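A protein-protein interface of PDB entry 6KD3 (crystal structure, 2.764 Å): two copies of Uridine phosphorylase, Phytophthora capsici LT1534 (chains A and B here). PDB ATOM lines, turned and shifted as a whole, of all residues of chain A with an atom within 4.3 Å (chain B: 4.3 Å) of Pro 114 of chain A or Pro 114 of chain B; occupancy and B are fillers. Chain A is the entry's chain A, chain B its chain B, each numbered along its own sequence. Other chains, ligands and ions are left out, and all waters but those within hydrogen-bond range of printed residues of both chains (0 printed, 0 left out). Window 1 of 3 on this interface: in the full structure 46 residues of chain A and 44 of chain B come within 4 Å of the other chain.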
ATOM      1  N   ILE A 111     -32.165  18.471   5.913  1.00  0.00           N
ATOM      2  CA  ILE A 111     -32.291  19.371   4.763  1.00  0.00           C
ATOM      3  C   ILE A 111     -31.568  18.773   3.567  1.00  0.00           C
ATOM      4  O   ILE A 111     -30.357  18.516   3.628  1.00  0.00           O
ATOM      5  CB  ILE A 111     -31.709  20.751   5.074  1.00  0.00           C
ATOM      6  CG1 ILE A 111     -31.856  21.671   3.883  1.00  0.00           C
ATOM      7  N   GLY A 112     -32.301  18.553   2.488  1.00  0.00           N
ATOM      8  CA  GLY A 112     -31.695  18.236   1.213  1.00  0.00           C
ATOM      9  C   GLY A 112     -31.283  16.779   1.107  1.00  0.00           C
ATOM     10  O   GLY A 112     -31.308  16.011   2.077  1.00  0.00           O
ATOM     11  N   MET A 113     -30.857  16.409  -0.117  1.00  0.00           N
ATOM     12  CA  MET A 113     -30.600  15.019  -0.486  1.00  0.00           C
ATOM     13  C   MET A 113     -29.713  14.237   0.496  1.00  0.00           C
ATOM     14  O   MET A 113     -30.200  13.254   1.087  1.00  0.00           O
ATOM     15  CB  MET A 113     -30.010  14.971  -1.897  1.00  0.00           C
ATOM     16  CG  MET A 113     -30.997  15.439  -2.958  1.00  0.00           C
ATOM     17  N   PRO A 114     -28.433  14.595   0.713  1.00  0.00           N
ATOM     18  CA  PRO A 114     -27.593  13.720   1.546  1.00  0.00           C
ATOM     19  C   PRO A 114     -28.159  13.517   2.936  1.00  0.00           C
ATOM     20  O   PRO A 114     -28.115  12.396   3.459  1.00  0.00           O
ATOM     21  CB  PRO A 114     -26.256  14.457   1.583  1.00  0.00           C
ATOM     22  CG  PRO A 114     -26.270  15.330   0.446  1.00  0.00           C
ATOM     23  CD  PRO A 114     -27.682  15.786   0.315  1.00  0.00           C
ATOM     24  N   SER A 115     -28.707  14.565   3.549  1.00  0.00           N
ATOM     25  CA  SER A 115     -29.385  14.373   4.823  1.00  0.00           C
ATOM     26  C   SER A 115     -30.450  13.299   4.692  1.00  0.00           C
ATOM     27  O   SER A 115     -30.505  12.357   5.488  1.00  0.00           O
ATOM     28  CB  SER A 115     -29.994  15.693   5.301  1.00  0.00           C
ATOM     29  OG  SER A 115     -30.633  15.540   6.548  1.00  0.00           O
ATOM     30  N   ILE A 116     -31.266  13.383   3.642  1.00  0.00           N
ATOM     31  CA  ILE A 116     -32.397  12.470   3.564  1.00  0.00           C
ATOM     32  C   ILE A 116     -32.013  11.092   3.039  1.00  0.00           C
ATOM     33  O   ILE A 116     -32.788  10.144   3.227  1.00  0.00           O
ATOM     34  CB  ILE A 116     -33.534  13.072   2.727  1.00  0.00           C
ATOM     35  CG1 ILE A 116     -34.845  12.388   3.099  1.00  0.00           C
ATOM     36  CG2 ILE A 116     -33.230  12.972   1.246  1.00  0.00           C
ATOM     37  CD1 ILE A 116     -36.034  12.832   2.282  1.00  0.00           C
ATOM     38  N   SER A 117     -30.828  10.931   2.425  1.00  0.00           N
ATOM     39  CA  SER A 117     -30.424   9.595   1.979  1.00  0.00           C
ATOM     40  C   SER A 117     -29.984   8.703   3.126  1.00  0.00           C
ATOM     41  O   SER A 117     -30.164   7.481   3.057  1.00  0.00           O
ATOM     42  CB  SER A 117     -29.282   9.639   0.980  1.00  0.00           C
ATOM     43  OG  SER A 117     -28.497   8.449   1.141  1.00  0.00           O
ATOM     44  N   ILE A 118     -29.359   9.260   4.153  1.00  0.00           N
ATOM     45  CA  ILE A 118     -28.932   8.426   5.265  1.00  0.00           C
ATOM     46  C   ILE A 118     -30.170   7.812   5.884  1.00  0.00           C
ATOM     47  O   ILE A 118     -30.376   6.601   5.771  1.00  0.00           O
ATOM     48  CB  ILE A 118     -28.139   9.228   6.294  1.00  0.00           C
ATOM     49  CG1 ILE A 118     -26.724   9.453   5.780  1.00  0.00           C
ATOM     50  CG2 ILE A 118     -28.126   8.496   7.613  1.00  0.00           C
ATOM     51  CD1 ILE A 118     -25.952  10.487   6.582  1.00  0.00           C
ATOM     52  N   ASN A 211     -30.562  21.040  -5.255  1.00  0.00           N
ATOM     53  CA  ASN A 211     -29.557  21.021  -4.203  1.00  0.00           C
ATOM     54  C   ASN A 211     -29.141  22.411  -3.726  1.00  0.00           C
ATOM     55  O   ASN A 211     -28.428  22.512  -2.722  1.00  0.00           O
ATOM     56  CB  ASN A 211     -28.322  20.231  -4.659  1.00  0.00           C
ATOM     57  CG  ASN A 211     -28.448  18.735  -4.385  1.00  0.00           C
ATOM     58  N   MET A 249     -36.231  20.141  -2.307  1.00  0.00           N
ATOM     59  CA  MET A 249     -34.824  19.730  -2.294  1.00  0.00           C
ATOM     60  C   MET A 249     -34.578  18.244  -2.024  1.00  0.00           C
ATOM     61  O   MET A 249     -33.487  17.756  -2.357  1.00  0.00           O
ATOM     62  CB  MET A 249     -34.030  20.515  -1.259  1.00  0.00           C
ATOM     63  CG  MET A 249     -34.414  21.991  -1.093  1.00  0.00           C
ATOM     64  SD  MET A 249     -32.980  22.796  -0.348  1.00  0.00           S
ATOM     65  CE  MET A 249     -32.366  21.575   0.802  1.00  0.00           C
ATOM     66  N   GLY B 112     -25.261  16.924   4.646  1.00  0.00           N
ATOM     67  CA  GLY B 112     -25.185  17.175   3.231  1.00  0.00           C
ATOM     68  C   GLY B 112     -24.661  18.551   2.908  1.00  0.00           C
ATOM     69  O   GLY B 112     -24.579  19.444   3.755  1.00  0.00           O
ATOM     70  N   MET B 113     -24.284  18.715   1.628  1.00  0.00           N
ATOM     71  CA  MET B 113     -24.032  20.033   1.042  1.00  0.00           C
ATOM     72  C   MET B 113     -25.314  20.868   0.951  1.00  0.00           C
ATOM     73  O   MET B 113     -25.253  22.085   1.196  1.00  0.00           O
ATOM     74  CB  MET B 113     -23.395  19.900  -0.339  1.00  0.00           C
ATOM     75  CG  MET B 113     -22.271  18.857  -0.399  1.00  0.00           C
ATOM     76  N   PRO B 114     -26.486  20.283   0.601  1.00  0.00           N
ATOM     77  CA  PRO B 114     -27.714  21.095   0.543  1.00  0.00           C
ATOM     78  C   PRO B 114     -28.016  21.872   1.804  1.00  0.00           C
ATOM     79  O   PRO B 114     -28.380  23.054   1.714  1.00  0.00           O
ATOM     80  CB  PRO B 114     -28.797  20.057   0.274  1.00  0.00           C
ATOM     81  CG  PRO B 114     -28.144  19.069  -0.508  1.00  0.00           C
ATOM     82  CD  PRO B 114     -26.719  18.976  -0.035  1.00  0.00           C
ATOM     83  N   SER B 115     -27.924  21.246   2.979  1.00  0.00           N
ATOM     84  CA  SER B 115     -28.218  21.990   4.197  1.00  0.00           C
ATOM     85  C   SER B 115     -27.201  23.090   4.389  1.00  0.00           C
ATOM     86  O   SER B 115     -27.555  24.255   4.593  1.00  0.00           O
ATOM     87  CB  SER B 115     -28.223  21.076   5.419  1.00  0.00           C
ATOM     88  OG  SER B 115     -28.527  21.818   6.587  1.00  0.00           O
ATOM     89  N   ILE B 116     -25.922  22.733   4.290  1.00  0.00           N
ATOM     90  CA  ILE B 116     -24.874  23.639   4.728  1.00  0.00           C
ATOM     91  C   ILE B 116     -24.841  24.891   3.858  1.00  0.00           C
ATOM     92  O   ILE B 116     -24.500  25.974   4.343  1.00  0.00           O
ATOM     93  CB  ILE B 116     -23.542  22.882   4.754  1.00  0.00           C
ATOM     94  CG1 ILE B 116     -22.494  23.650   5.559  1.00  0.00           C
ATOM     95  CG2 ILE B 116     -23.098  22.569   3.347  1.00  0.00           C
ATOM     96  CD1 ILE B 116     -21.062  23.045   5.471  1.00  0.00           C
ATOM     97  N   SER B 117     -25.268  24.792   2.592  1.00  0.00           N
ATOM     98  CA  SER B 117     -25.324  25.984   1.740  1.00  0.00           C
ATOM     99  C   SER B 117     -26.449  26.941   2.129  1.00  0.00           C
ATOM    100  O   SER B 117     -26.395  28.114   1.766  1.00  0.00           O
ATOM    101  CB  SER B 117     -25.469  25.596   0.263  1.00  0.00           C
ATOM    102  OG  SER B 117     -24.901  26.593  -0.573  1.00  0.00           O
ATOM    103  N   ILE B 118     -27.457  26.479   2.857  1.00  0.00           N
ATOM    104  CA  ILE B 118     -28.519  27.383   3.282  1.00  0.00           C
ATOM    105  C   ILE B 118     -28.069  28.202   4.480  1.00  0.00           C
ATOM    106  O   ILE B 118     -28.380  29.387   4.599  1.00  0.00           O
ATOM    107  CB  ILE B 118     -29.796  26.586   3.603  1.00  0.00           C
ATOM    108  CG1 ILE B 118     -30.253  25.781   2.382  1.00  0.00           C
ATOM    109  CG2 ILE B 118     -30.891  27.509   4.081  1.00  0.00           C
ATOM    110  CD1 ILE B 118     -31.430  24.924   2.658  1.00  0.00           C
ATOM    111  N   ASN B 211     -22.154  13.311  -1.990  1.00  0.00           N
ATOM    112  CA  ASN B 211     -23.553  13.627  -1.725  1.00  0.00           C
ATOM    113  C   ASN B 211     -24.341  12.442  -1.161  1.00  0.00           C
ATOM    114  O   ASN B 211     -25.490  12.636  -0.754  1.00  0.00           O
ATOM    115  CB  ASN B 211     -24.191  14.158  -2.978  1.00  0.00           C
ATOM    116  CG  ASN B 211     -23.769  15.573  -3.280  1.00  0.00           C
ATOM    117  N   MET B 249     -19.223  15.063   3.987  1.00  0.00           N
ATOM    118  CA  MET B 249     -20.105  15.365   2.864  1.00  0.00           C
ATOM    119  C   MET B 249     -20.591  16.806   2.822  1.00  0.00           C
ATOM    120  O   MET B 249     -21.637  17.075   2.212  1.00  0.00           O
ATOM    121  CB  MET B 249     -21.312  14.435   2.866  1.00  0.00           C
ATOM    122  CG  MET B 249     -21.710  13.947   4.236  1.00  0.00           C
ATOM    123  SD  MET B 249     -23.276  13.077   4.125  1.00  0.00           S
ATOM    124  CE  MET B 249     -22.843  11.874   2.883  1.00  0.00           C
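N of Ile 111 of chain A lies within hydrogen-bond range of OG of Ser 115 of chain A.
Ser 115 of chain B touches Ile 111 of chain A. Ile 118 of chain B touches Ile 111 of chain A. CA of Gly 112 of chain A touches CB of Pro 114 of chain B, at 3.5 Å. Met 113 of chain A touches Pro 114 of chain B (N to CG, 3.8 Å). Gly 112 of chain B touches Pro 114 of chain A (CA to CB, 3.4 Å). Pro 114 of chain A touches Pro 114 of chain B. Asn 211 of chain B touches Pro 114 of chain A. Pro 114 of chain B touches Asn 211 of chain A (CA to O, 3.6 Å). CB of Pro 114 of chain B touches CE of Met 249 of chain A (3.9 Å). CD1 of Ile 118 of chain B touches CE of Met 249 of chain A (3.9 Å).
Of chain B, only Gly 112 (3.4 Å), Pro 114 (3.4 Å) and Asn 211 (3.1 Å) come within 4 Å of Pro 114 of chain A. Of the printed residues of chain A, Pro 114 of chain B touches Gly 112, Met 113, Pro 114, Asn 211 and Met 249. Of the printed residues of chain B, Asn 211 of chain A touches Pro 114 (3.6 Å). Printed residues of chain A within 4 Å of Ile 118 of chain B: Ile 111 (3.5 Å) and Met 249 (3.9 Å). Of the printed residues of chain B, Met 113 of chain A touches Pro 114 (3.8 Å). Printed residues of chain A within 4 Å of Gly 112 of chain B: Pro 114. Of the printed residues of chain A, Ser 115 of chain B touches Ile 111 (3.5 Å). Ser 117 of chain A touches none of the printed residues of chain B. Ser 115 of chain A touches none of the printed residues of chain B. The nearest residue of chain B that does not touch Pro 114 of chain A is Met 113 of chain B (4.1 Å). The nearest printed residue of chain A that does not touch Pro 114 of chain B is Ile 111 of chain A (4.01 Å). The nearest printed residue of chain A that does not touch Ile 118 of chain B is Asn 211 of chain A (6.3 Å).
Hydrophobic or aromatic side chains of chain A within 4 Å of the printed part of chain B: Ile 111, Pro 114 and Met 249. Of the 9 printed residues of chain B, 5 touch a printed residue of chain A. Hydrophobic or aromatic side chains of chain B within 4 Å of the printed part of chain A: Pro 114 and Ile 118. Among the printed residues, no Asp or Glu carboxylate lies within 4 Å of a Lys or Arg side-chain nitrogen of the other chain.
Gly 112 of chain A touches Pro 114 of chain B, and with the chains exchanged Pro 114 of chain A touches Gly 112 of chain B. Met 113 of chain A touches Pro 114 of chain B, but with the chains exchanged Pro 114 of chain A does not touch Met 113 of chain B (4.1 Å). Pro 114 of chain A touches Asn 211 of chain B, and with the chains exchanged Asn 211 of chain A touches Pro 114 of chain B. Met 249 of chain A touches Pro 114 of chain B, but with the chains exchanged Pro 114 of chain A does not touch Met 249 of chain B (4.2 Å). Positions printed for both chains: 112, 113, 114, 115, 116, 117, 118, 211 and 249. Of the 10 pairs that touch across the chains among the printed residues, 5 have their exchanged pair printed and touching as well.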
